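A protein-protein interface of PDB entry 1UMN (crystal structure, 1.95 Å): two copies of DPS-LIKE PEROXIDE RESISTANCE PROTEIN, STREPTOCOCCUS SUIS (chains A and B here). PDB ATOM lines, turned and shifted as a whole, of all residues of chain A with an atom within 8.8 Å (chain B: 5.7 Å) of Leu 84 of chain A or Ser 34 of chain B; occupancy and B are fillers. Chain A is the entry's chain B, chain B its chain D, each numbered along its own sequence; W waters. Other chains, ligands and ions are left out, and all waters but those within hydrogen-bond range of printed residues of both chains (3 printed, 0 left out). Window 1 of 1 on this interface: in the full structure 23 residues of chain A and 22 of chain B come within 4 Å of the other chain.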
ATOM      1  N   ALA A  27     -23.261  22.930 -14.576  1.00  0.00           N
ATOM      2  CA  ALA A  27     -21.996  23.646 -14.555  1.00  0.00           C
ATOM      3  C   ALA A  27     -20.789  22.705 -14.528  1.00  0.00           C
ATOM      4  O   ALA A  27     -19.860  22.875 -15.313  1.00  0.00           O
ATOM      5  CB  ALA A  27     -21.955  24.623 -13.347  1.00  0.00           C
ATOM      6  N   SER A  30     -20.293  20.730 -17.720  1.00  0.00           N
ATOM      7  CA  SER A  30     -19.768  21.596 -18.783  1.00  0.00           C
ATOM      8  C   SER A  30     -18.249  21.743 -18.655  1.00  0.00           C
ATOM      9  O   SER A  30     -17.510  21.677 -19.653  1.00  0.00           O
ATOM     10  CB  SER A  30     -20.429  22.988 -18.744  1.00  0.00           C
ATOM     11  OG  SER A  30     -21.819  22.917 -19.040  1.00  0.00           O
ATOM     12  N   VAL A  31     -17.775  21.939 -17.430  1.00  0.00           N
ATOM     13  CA  VAL A  31     -16.346  22.071 -17.229  1.00  0.00           C
ATOM     14  C   VAL A  31     -15.674  20.710 -17.417  1.00  0.00           C
ATOM     15  O   VAL A  31     -14.585  20.622 -17.995  1.00  0.00           O
ATOM     16  CB  VAL A  31     -16.029  22.667 -15.836  1.00  0.00           C
ATOM     17  CG1 VAL A  31     -14.536  22.617 -15.571  1.00  0.00           C
ATOM     18  CG2 VAL A  31     -16.505  24.131 -15.785  1.00  0.00           C
ATOM     19  N   SER A  34     -15.036  20.152 -21.007  1.00  0.00           N
ATOM     20  CA  SER A  34     -13.903  20.955 -21.451  1.00  0.00           C
ATOM     21  C   SER A  34     -12.558  20.299 -21.091  1.00  0.00           C
ATOM     22  O   SER A  34     -11.628  20.294 -21.894  1.00  0.00           O
ATOM     23  CB  SER A  34     -13.973  22.354 -20.818  1.00  0.00           C
ATOM     24  OG  SER A  34     -12.910  23.179 -21.269  1.00  0.00           O
ATOM     25  N   LEU A  66     -25.595  15.895 -19.337  1.00  0.00           N
ATOM     26  CA  LEU A  66     -25.953  17.313 -19.365  1.00  0.00           C
ATOM     27  C   LEU A  66     -27.349  17.446 -19.990  1.00  0.00           C
ATOM     28  O   LEU A  66     -28.163  18.254 -19.535  1.00  0.00           O
ATOM     29  CB  LEU A  66     -24.913  18.106 -20.160  1.00  0.00           C
ATOM     30  CG  LEU A  66     -25.202  19.582 -20.463  1.00  0.00           C
ATOM     31  CD1 LEU A  66     -25.476  20.361 -19.190  1.00  0.00           C
ATOM     32  CD2 LEU A  66     -23.997  20.176 -21.189  1.00  0.00           C
ATOM     33  N   PHE A  81     -27.830  27.293 -16.042  1.00  0.00           N
ATOM     34  CA  PHE A  81     -26.679  28.147 -16.308  1.00  0.00           C
ATOM     35  C   PHE A  81     -26.534  27.883 -17.807  1.00  0.00           C
ATOM     36  O   PHE A  81     -26.743  26.749 -18.254  1.00  0.00           O
ATOM     37  CB  PHE A  81     -25.441  27.612 -15.574  1.00  0.00           C
ATOM     38  CG  PHE A  81     -25.506  27.760 -14.081  1.00  0.00           C
ATOM     39  CD1 PHE A  81     -25.178  26.688 -13.247  1.00  0.00           C
ATOM     40  CD2 PHE A  81     -25.889  28.965 -13.506  1.00  0.00           C
ATOM     41  CE1 PHE A  81     -25.235  26.814 -11.852  1.00  0.00           C
ATOM     42  CE2 PHE A  81     -25.952  29.114 -12.113  1.00  0.00           C
ATOM     43  CZ  PHE A  81     -25.626  28.030 -11.281  1.00  0.00           C
ATOM     44  N   SER A  82     -26.189  28.900 -18.589  1.00  0.00           N
ATOM     45  CA  SER A  82     -26.095  28.682 -20.026  1.00  0.00           C
ATOM     46  C   SER A  82     -25.096  29.616 -20.701  1.00  0.00           C
ATOM     47  O   SER A  82     -25.306  30.038 -21.837  1.00  0.00           O
ATOM     48  CB  SER A  82     -27.494  28.844 -20.655  1.00  0.00           C
ATOM     49  OG  SER A  82     -28.018  30.158 -20.427  1.00  0.00           O
ATOM     50  N   THR A  83     -24.015  29.930 -19.988  1.00  0.00           N
ATOM     51  CA  THR A  83     -22.947  30.790 -20.491  1.00  0.00           C
ATOM     52  C   THR A  83     -21.640  30.209 -19.930  1.00  0.00           C
ATOM     53  O   THR A  83     -21.651  29.600 -18.871  1.00  0.00           O
ATOM     54  CB  THR A  83     -23.092  32.257 -19.984  1.00  0.00           C
ATOM     55  OG1 THR A  83     -23.041  32.271 -18.550  1.00  0.00           O
ATOM     56  CG2 THR A  83     -24.425  32.874 -20.459  1.00  0.00           C
ATOM     57  N   LEU A  84     -20.526  30.388 -20.629  1.00  0.00           N
ATOM     58  CA  LEU A  84     -19.248  29.855 -20.145  1.00  0.00           C
ATOM     59  C   LEU A  84     -18.868  30.439 -18.774  1.00  0.00           C
ATOM     60  O   LEU A  84     -18.311  29.730 -17.913  1.00  0.00           O
ATOM     61  CB  LEU A  84     -18.138  30.118 -21.171  1.00  0.00           C
ATOM     62  CG  LEU A  84     -18.372  29.516 -22.567  1.00  0.00           C
ATOM     63  CD1 LEU A  84     -17.048  29.490 -23.333  1.00  0.00           C
ATOM     64  CD2 LEU A  84     -18.909  28.091 -22.444  1.00  0.00           C
ATOM     65  N   LYS A  85     -19.174  31.717 -18.567  1.00  0.00           N
ATOM     66  CA  LYS A  85     -18.874  32.373 -17.287  1.00  0.00           C
ATOM     67  C   LYS A  85     -19.578  31.655 -16.130  1.00  0.00           C
ATOM     68  O   LYS A  85     -18.963  31.336 -15.106  1.00  0.00           O
ATOM     69  CB  LYS A  85     -19.329  33.834 -17.295  1.00  0.00           C
ATOM     70  CG  LYS A  85     -19.147  34.520 -15.944  1.00  0.00           C
ATOM     71  CD  LYS A  85     -19.812  35.892 -15.910  1.00  0.00           C
ATOM     72  CE  LYS A  85     -19.634  36.577 -14.530  1.00  0.00           C
ATOM     73  NZ  LYS A  85     -18.192  36.675 -14.148  1.00  0.00           N
ATOM     74  N   GLU A  86     -20.872  31.409 -16.293  1.00  0.00           N
ATOM     75  CA  GLU A  86     -21.646  30.735 -15.255  1.00  0.00           C
ATOM     76  C   GLU A  86     -21.117  29.321 -15.003  1.00  0.00           C
ATOM     77  O   GLU A  86     -21.024  28.862 -13.858  1.00  0.00           O
ATOM     78  CB  GLU A  86     -23.119  30.661 -15.663  1.00  0.00           C
ATOM     79  CG  GLU A  86     -23.848  31.993 -15.667  1.00  0.00           C
ATOM     80  CD  GLU A  86     -25.272  31.824 -16.147  1.00  0.00           C
ATOM     81  OE1 GLU A  86     -26.194  31.906 -15.316  1.00  0.00           O
ATOM     82  OE2 GLU A  86     -25.456  31.579 -17.356  1.00  0.00           O
ATOM     83  N   PHE A  87     -20.798  28.614 -16.079  1.00  0.00           N
ATOM     84  CA  PHE A  87     -20.278  27.261 -15.950  1.00  0.00           C
ATOM     85  C   PHE A  87     -18.981  27.287 -15.139  1.00  0.00           C
ATOM     86  O   PHE A  87     -18.856  26.608 -14.129  1.00  0.00           O
ATOM     87  CB  PHE A  87     -19.965  26.665 -17.326  1.00  0.00           C
ATOM     88  CG  PHE A  87     -21.167  26.465 -18.213  1.00  0.00           C
ATOM     89  CD1 PHE A  87     -21.002  26.388 -19.598  1.00  0.00           C
ATOM     90  CD2 PHE A  87     -22.446  26.300 -17.677  1.00  0.00           C
ATOM     91  CE1 PHE A  87     -22.086  26.150 -20.432  1.00  0.00           C
ATOM     92  CE2 PHE A  87     -23.543  26.060 -18.504  1.00  0.00           C
ATOM     93  CZ  PHE A  87     -23.367  25.984 -19.886  1.00  0.00           C
ATOM     94  N   SER A  88     -18.025  28.085 -15.607  1.00  0.00           N
ATOM     95  CA  SER A  88     -16.717  28.185 -14.980  1.00  0.00           C
ATOM     96  C   SER A  88     -16.773  28.595 -13.510  1.00  0.00           C
ATOM     97  O   SER A  88     -16.134  27.975 -12.657  1.00  0.00           O
ATOM     98  CB  SER A  88     -15.853  29.170 -15.770  1.00  0.00           C
ATOM     99  OG  SER A  88     -14.515  29.201 -15.296  1.00  0.00           O
ATOM    100  N   GLU A  89     -17.547  29.627 -13.212  1.00  0.00           N
ATOM    101  CA  GLU A  89     -17.660  30.117 -11.847  1.00  0.00           C
ATOM    102  C   GLU A  89     -18.397  29.202 -10.872  1.00  0.00           C
ATOM    103  O   GLU A  89     -17.994  29.080  -9.713  1.00  0.00           O
ATOM    104  CB  GLU A  89     -18.306  31.500 -11.857  1.00  0.00           C
ATOM    105  CG  GLU A  89     -17.366  32.550 -12.445  1.00  0.00           C
ATOM    106  CD  GLU A  89     -17.941  33.962 -12.440  1.00  0.00           C
ATOM    107  OE1 GLU A  89     -17.197  34.882 -12.851  1.00  0.00           O
ATOM    108  OE2 GLU A  89     -19.125  34.145 -12.039  1.00  0.00           O
ATOM    109  N   ASN A  90     -19.462  28.548 -11.326  1.00  0.00           N
ATOM    110  CA  ASN A  90     -20.213  27.674 -10.435  1.00  0.00           C
ATOM    111  C   ASN A  90     -19.634  26.271 -10.285  1.00  0.00           C
ATOM    112  O   ASN A  90     -19.867  25.603  -9.279  1.00  0.00           O
ATOM    113  CB  ASN A  90     -21.668  27.593 -10.901  1.00  0.00           C
ATOM    114  CG  ASN A  90     -22.442  28.867 -10.595  1.00  0.00           C
ATOM    115  OD1 ASN A  90     -22.871  29.073  -9.465  1.00  0.00           O
ATOM    116  ND2 ASN A  90     -22.602  29.735 -11.593  1.00  0.00           N
ATOM    117  N   SER A  91     -18.883  25.818 -11.282  1.00  0.00           N
ATOM    118  CA  SER A  91     -18.293  24.486 -11.205  1.00  0.00           C
ATOM    119  C   SER A  91     -17.234  24.458 -10.116  1.00  0.00           C
ATOM    120  O   SER A  91     -16.560  25.465  -9.881  1.00  0.00           O
ATOM    121  CB  SER A  91     -17.626  24.116 -12.531  1.00  0.00           C
ATOM    122  OG  SER A  91     -16.988  22.852 -12.425  1.00  0.00           O
ATOM    123  N   GLU A  95      -9.734  24.268 -14.070  1.00  0.00           N
ATOM    124  CA  GLU A  95      -9.052  24.000 -15.329  1.00  0.00           C
ATOM    125  C   GLU A  95      -7.703  24.678 -15.366  1.00  0.00           C
ATOM    126  O   GLU A  95      -7.528  25.757 -14.785  1.00  0.00           O
ATOM    127  CB  GLU A  95      -9.870  24.514 -16.502  1.00  0.00           C
ATOM    128  CG  GLU A  95     -11.297  24.000 -16.548  1.00  0.00           C
ATOM    129  CD  GLU A  95     -11.969  24.401 -17.839  1.00  0.00           C
ATOM    130  OE1 GLU A  95     -11.808  23.667 -18.842  1.00  0.00           O
ATOM    131  OE2 GLU A  95     -12.630  25.460 -17.849  1.00  0.00           O
ATOM    132  N   LEU B  29     -16.043  29.064 -31.831  1.00  0.00           N
ATOM    133  CA  LEU B  29     -16.928  27.909 -31.990  1.00  0.00           C
ATOM    134  C   LEU B  29     -17.399  27.382 -30.625  1.00  0.00           C
ATOM    135  O   LEU B  29     -18.538  26.922 -30.485  1.00  0.00           O
ATOM    136  CB  LEU B  29     -16.218  26.790 -32.782  1.00  0.00           C
ATOM    137  CG  LEU B  29     -16.028  27.105 -34.280  1.00  0.00           C
ATOM    138  CD1 LEU B  29     -15.043  26.128 -34.926  1.00  0.00           C
ATOM    139  CD2 LEU B  29     -17.396  27.051 -34.992  1.00  0.00           C
ATOM    140  N   SER B  30     -16.522  27.431 -29.624  1.00  0.00           N
ATOM    141  CA  SER B  30     -16.895  26.977 -28.289  1.00  0.00           C
ATOM    142  C   SER B  30     -17.959  27.917 -27.723  1.00  0.00           C
ATOM    143  O   SER B  30     -18.919  27.463 -27.103  1.00  0.00           O
ATOM    144  CB  SER B  30     -15.665  26.944 -27.363  1.00  0.00           C
ATOM    145  OG  SER B  30     -14.668  26.055 -27.874  1.00  0.00           O
ATOM    146  N   VAL B  31     -17.805  29.223 -27.933  1.00  0.00           N
ATOM    147  CA  VAL B  31     -18.810  30.152 -27.426  1.00  0.00           C
ATOM    148  C   VAL B  31     -20.105  30.026 -28.231  1.00  0.00           C
ATOM    149  O   VAL B  31     -21.193  30.040 -27.665  1.00  0.00           O
ATOM    150  CB  VAL B  31     -18.297  31.603 -27.447  1.00  0.00           C
ATOM    151  CG1 VAL B  31     -19.396  32.570 -26.966  1.00  0.00           C
ATOM    152  CG2 VAL B  31     -17.084  31.715 -26.512  1.00  0.00           C
ATOM    153  N   ALA B  32     -19.986  29.869 -29.551  1.00  0.00           N
ATOM    154  CA  ALA B  32     -21.176  29.709 -30.395  1.00  0.00           C
ATOM    155  C   ALA B  32     -21.971  28.479 -29.947  1.00  0.00           C
ATOM    156  O   ALA B  32     -23.208  28.505 -29.890  1.00  0.00           O
ATOM    157  CB  ALA B  32     -20.770  29.561 -31.874  1.00  0.00           C
ATOM    158  N   HIS B  33     -21.265  27.394 -29.637  1.00  0.00           N
ATOM    159  CA  HIS B  33     -21.931  26.160 -29.206  1.00  0.00           C
ATOM    160  C   HIS B  33     -22.734  26.427 -27.932  1.00  0.00           C
ATOM    161  O   HIS B  33     -23.857  25.943 -27.774  1.00  0.00           O
ATOM    162  CB  HIS B  33     -20.889  25.050 -28.942  1.00  0.00           C
ATOM    163  CG  HIS B  33     -21.492  23.708 -28.637  1.00  0.00           C
ATOM    164  ND1 HIS B  33     -21.629  22.716 -29.585  1.00  0.00           N
ATOM    165  CD2 HIS B  33     -22.015  23.207 -27.494  1.00  0.00           C
ATOM    166  CE1 HIS B  33     -22.210  21.661 -29.039  1.00  0.00           C
ATOM    167  NE2 HIS B  33     -22.455  21.935 -27.769  1.00  0.00           N
ATOM    168  N   SER B  34     -22.142  27.203 -27.031  1.00  0.00           N
ATOM    169  CA  SER B  34     -22.782  27.545 -25.770  1.00  0.00           C
ATOM    170  C   SER B  34     -24.032  28.393 -26.011  1.00  0.00           C
ATOM    171  O   SER B  34     -25.082  28.172 -25.387  1.00  0.00           O
ATOM    172  CB  SER B  34     -21.791  28.293 -24.872  1.00  0.00           C
ATOM    173  OG  SER B  34     -22.393  28.619 -23.625  1.00  0.00           O
ATOM    174  N   ILE B  35     -23.933  29.344 -26.931  1.00  0.00           N
ATOM    175  CA  ILE B  35     -25.068  30.205 -27.250  1.00  0.00           C
ATOM    176  C   ILE B  35     -26.195  29.363 -27.849  1.00  0.00           C
ATOM    177  O   ILE B  35     -27.368  29.498 -27.469  1.00  0.00           O
ATOM    178  CB  ILE B  35     -24.643  31.329 -28.238  1.00  0.00           C
ATOM    179  CG1 ILE B  35     -23.686  32.304 -27.530  1.00  0.00           C
ATOM    180  CG2 ILE B  35     -25.869  32.082 -28.732  1.00  0.00           C
ATOM    181  CD1 ILE B  35     -23.057  33.351 -28.459  1.00  0.00           C
ATOM    182  N   LEU B  36     -25.838  28.471 -28.766  1.00  0.00           N
ATOM    183  CA  LEU B  36     -26.844  27.618 -29.372  1.00  0.00           C
ATOM    184  C   LEU B  36     -27.537  26.758 -28.311  1.00  0.00           C
ATOM    185  O   LEU B  36     -28.735  26.507 -28.408  1.00  0.00           O
ATOM    186  CB  LEU B  36     -26.223  26.703 -30.434  1.00  0.00           C
ATOM    187  CG  LEU B  36     -25.740  27.377 -31.729  1.00  0.00           C
ATOM    188  CD1 LEU B  36     -24.913  26.382 -32.571  1.00  0.00           C
ATOM    189  CD2 LEU B  36     -26.938  27.892 -32.514  1.00  0.00           C
ATOM    190  N   HIS B  37     -26.784  26.302 -27.309  1.00  0.00           N
ATOM    191  CA  HIS B  37     -27.372  25.468 -26.272  1.00  0.00           C
ATOM    192  C   HIS B  37     -28.377  26.296 -25.486  1.00  0.00           C
ATOM    193  O   HIS B  37     -29.450  25.809 -25.121  1.00  0.00           O
ATOM    194  CB  HIS B  37     -26.303  24.914 -25.325  1.00  0.00           C
ATOM    195  CG  HIS B  37     -26.573  23.506 -24.888  1.00  0.00           C
ATOM    196  ND1 HIS B  37     -27.827  22.936 -24.956  1.00  0.00           N
ATOM    197  CD2 HIS B  37     -25.751  22.546 -24.403  1.00  0.00           C
ATOM    198  CE1 HIS B  37     -27.766  21.684 -24.536  1.00  0.00           C
ATOM    199  NE2 HIS B  37     -26.519  21.424 -24.194  1.00  0.00           N
ATOM    200  N   GLN B  38     -28.021  27.549 -25.218  1.00  0.00           N
ATOM    201  CA  GLN B  38     -28.927  28.439 -24.506  1.00  0.00           C
ATOM    202  C   GLN B  38     -30.225  28.604 -25.310  1.00  0.00           C
ATOM    203  O   GLN B  38     -31.323  28.519 -24.756  1.00  0.00           O
ATOM    204  CB  GLN B  38     -28.278  29.799 -24.310  1.00  0.00           C
ATOM    205  CG  GLN B  38     -29.148  30.769 -23.525  1.00  0.00           C
ATOM    206  CD  GLN B  38     -28.464  32.101 -23.348  1.00  0.00           C
ATOM    207  OE1 GLN B  38     -28.573  32.998 -24.202  1.00  0.00           O
ATOM    208  NE2 GLN B  38     -27.718  32.235 -22.252  1.00  0.00           N
ATOM    209  N   VAL B  39     -30.108  28.842 -26.616  1.00  0.00           N
ATOM    210  CA  VAL B  39     -31.302  29.007 -27.456  1.00  0.00           C
ATOM    211  C   VAL B  39     -32.172  27.744 -27.392  1.00  0.00           C
ATOM    212  O   VAL B  39     -33.403  27.805 -27.296  1.00  0.00           O
ATOM    213  CB  VAL B  39     -30.912  29.271 -28.929  1.00  0.00           C
ATOM    214  CG1 VAL B  39     -32.166  29.276 -29.818  1.00  0.00           C
ATOM    215  CG2 VAL B  39     -30.172  30.617 -29.024  1.00  0.00           C
ATOM    216  N   LEU B  84     -12.591  26.929 -20.423  1.00  0.00           N
ATOM    217  CA  LEU B  84     -13.704  27.844 -20.659  1.00  0.00           C
ATOM    218  C   LEU B  84     -13.296  29.319 -20.592  1.00  0.00           C
ATOM    219  O   LEU B  84     -13.797  30.131 -21.370  1.00  0.00           O
ATOM    220  CB  LEU B  84     -14.860  27.558 -19.686  1.00  0.00           C
ATOM    221  CG  LEU B  84     -15.456  26.144 -19.699  1.00  0.00           C
ATOM    222  CD1 LEU B  84     -16.775  26.160 -18.941  1.00  0.00           C
ATOM    223  CD2 LEU B  84     -15.693  25.664 -21.129  1.00  0.00           C
ATOM    224  N   PHE B  87     -11.699  30.271 -23.911  1.00  0.00           N
ATOM    225  CA  PHE B  87     -12.706  30.364 -24.962  1.00  0.00           C
ATOM    226  C   PHE B  87     -13.426  31.703 -24.840  1.00  0.00           C
ATOM    227  O   PHE B  87     -13.541  32.456 -25.809  1.00  0.00           O
ATOM    228  CB  PHE B  87     -13.753  29.250 -24.820  1.00  0.00           C
ATOM    229  CG  PHE B  87     -13.214  27.855 -25.009  1.00  0.00           C
ATOM    230  CD1 PHE B  87     -13.886  26.765 -24.462  1.00  0.00           C
ATOM    231  CD2 PHE B  87     -12.055  27.624 -25.746  1.00  0.00           C
ATOM    232  CE1 PHE B  87     -13.414  25.467 -24.644  1.00  0.00           C
ATOM    233  CE2 PHE B  87     -11.575  26.322 -25.936  1.00  0.00           C
ATOM    234  CZ  PHE B  87     -12.257  25.247 -25.384  1.00  0.00           C
ATOM    235  N   SER B  88     -13.900  31.988 -23.627  1.00  0.00           N
ATOM    236  CA  SER B  88     -14.668  33.195 -23.363  1.00  0.00           C
ATOM    237  C   SER B  88     -13.916  34.500 -23.587  1.00  0.00           C
ATOM    238  O   SER B  88     -14.450  35.443 -24.185  1.00  0.00           O
ATOM    239  CB  SER B  88     -15.220  33.158 -21.931  1.00  0.00           C
ATOM    240  OG  SER B  88     -16.138  34.223 -21.706  1.00  0.00           O
ATOM    241  N   GLU B  95     -21.833  36.599 -24.635  1.00  0.00           N
ATOM    242  CA  GLU B  95     -22.926  35.793 -24.092  1.00  0.00           C
ATOM    243  C   GLU B  95     -23.751  36.597 -23.106  1.00  0.00           C
ATOM    244  O   GLU B  95     -23.242  37.504 -22.446  1.00  0.00           O
ATOM    245  CB  GLU B  95     -22.395  34.542 -23.388  1.00  0.00           C
ATOM    246  CG  GLU B  95     -21.664  33.565 -24.310  1.00  0.00           C
ATOM    247  CD  GLU B  95     -21.331  32.257 -23.612  1.00  0.00           C
ATOM    248  OE1 GLU B  95     -22.138  31.309 -23.722  1.00  0.00           O
ATOM    249  OE2 GLU B  95     -20.280  32.186 -22.944  1.00  0.00           O
HETATM  250  O   HOH W   1     -24.605  31.625 -24.128  1.00  0.00           O
HETATM  251  O   HOH W   2     -24.540  27.056 -22.843  1.00  0.00           O
HETATM  252  O   HOH W   3     -11.406  28.105 -17.528  1.00  0.00           O
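The side-chain amide nitrogen (NE2) of Gln 38 of chain B sits at hydrogen-bond distance from the side-chain hydroxyl (OG) of Ser 82 of chain A (2.8 Å). OE2 of Glu 95 of chain B sits at hydrogen-bond distance from N of Leu 84 of chain A. OE2 of Glu 95 of chain A is in hydrogen-bond range of N of Leu 84 of chain B (3.0 Å).
OG of Ser 34 of chain A sits at hydrogen-bond distance from OE1 of Glu 95 of chain A, at 2.7 Å. OE2 of Glu 86 of chain A lies within hydrogen-bond range of N of Ser 82 of chain A, at 3.0 Å. OE2 of Glu 86 of chain A is in hydrogen-bond range of OG1 of Thr 83 of chain A. The side-chain carboxylate (OE1) of Glu 95 of chain B sits at hydrogen-bond distance from the side-chain hydroxyl (OG) of Ser 34 of chain B.
Among the printed residues, merely in contact across the chains: Val 31 of chain A with Leu 84 of chain B, Ser 34 of chain A with Leu 84 of chain B, Ser 82 of chain A with Ser 34 of chain B, Ser 82 of chain A with Glu 95 of chain B, Thr 83 of chain A with Ser 34 of chain B, Thr 83 of chain A with Gln 38 of chain B, Thr 83 of chain A with Glu 95 of chain B, Leu 84 of chain A with Val 31 of chain B, Leu 84 of chain A with Ser 34 of chain B, Leu 84 of chain A with Leu 84 of chain B, Leu 84 of chain A with Phe 87 of chain B and Phe 87 of chain A with Leu 84 of chain B.
Printed residues of chain B within 4 Å of Thr 83 of chain A: Ser 34, Gln 38 and Glu 95. Of chain B, only Val 31 (3.9 Å), Ser 34 (3.7 Å), Leu 84 (3.9 Å), Phe 87 (3.6 Å) and Glu 95 (2.9 Å) come within 4 Å of Leu 84 of chain A. Ser 88 of chain A touches none of the printed residues of chain B. Ser 91 of chain A touches none of the printed residues of chain B. Printed residues of chain A within 4 Å of Gln 38 of chain B: Ser 82 (2.8 Å) and Thr 83 (3.8 Å).
Hydrophobic or aromatic side chains of chain A within 4 Å of the printed part of chain B: Val 31, Leu 84 and Phe 87. Among the printed residues, 15 pairs touch across the chains. Among the printed residues, no Asp or Glu carboxylate lies within 4 Å of a Lys or Arg side-chain nitrogen of the other chain.
Val 31 of chain A touches Leu 84 of chain B, and with the chains exchanged Leu 84 of chain A touches Val 31 of chain B. Ser 34 of chain A touches Leu 84 of chain B, and with the chains exchanged Leu 84 of chain A touches Ser 34 of chain B. Leu 84 of chain B touches its own counterpart, Leu 84 of chain A. Leu 84 of chain A touches Phe 87 of chain B, and with the chains exchanged Phe 87 of chain A touches Leu 84 of chain B. Of the 15 pairs that touch across the chains among the printed residues, 9 have their exchanged pair printed and touching as well.
Water W1 bridges OE1 of Glu 95 of chain B (2.5 Å) and O of Ser 82 of chain A (2.9 Å). Water W2 bridges OG of Ser 34 of chain B and O of Ser 82 of chain A. Water W3 lies within hydrogen-bond range of the side-chain carboxylate (OE2) of Glu 95 of chain A (2.9 Å) and the backbone NH (N) of Leu 84 of chain B (3.3 Å).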
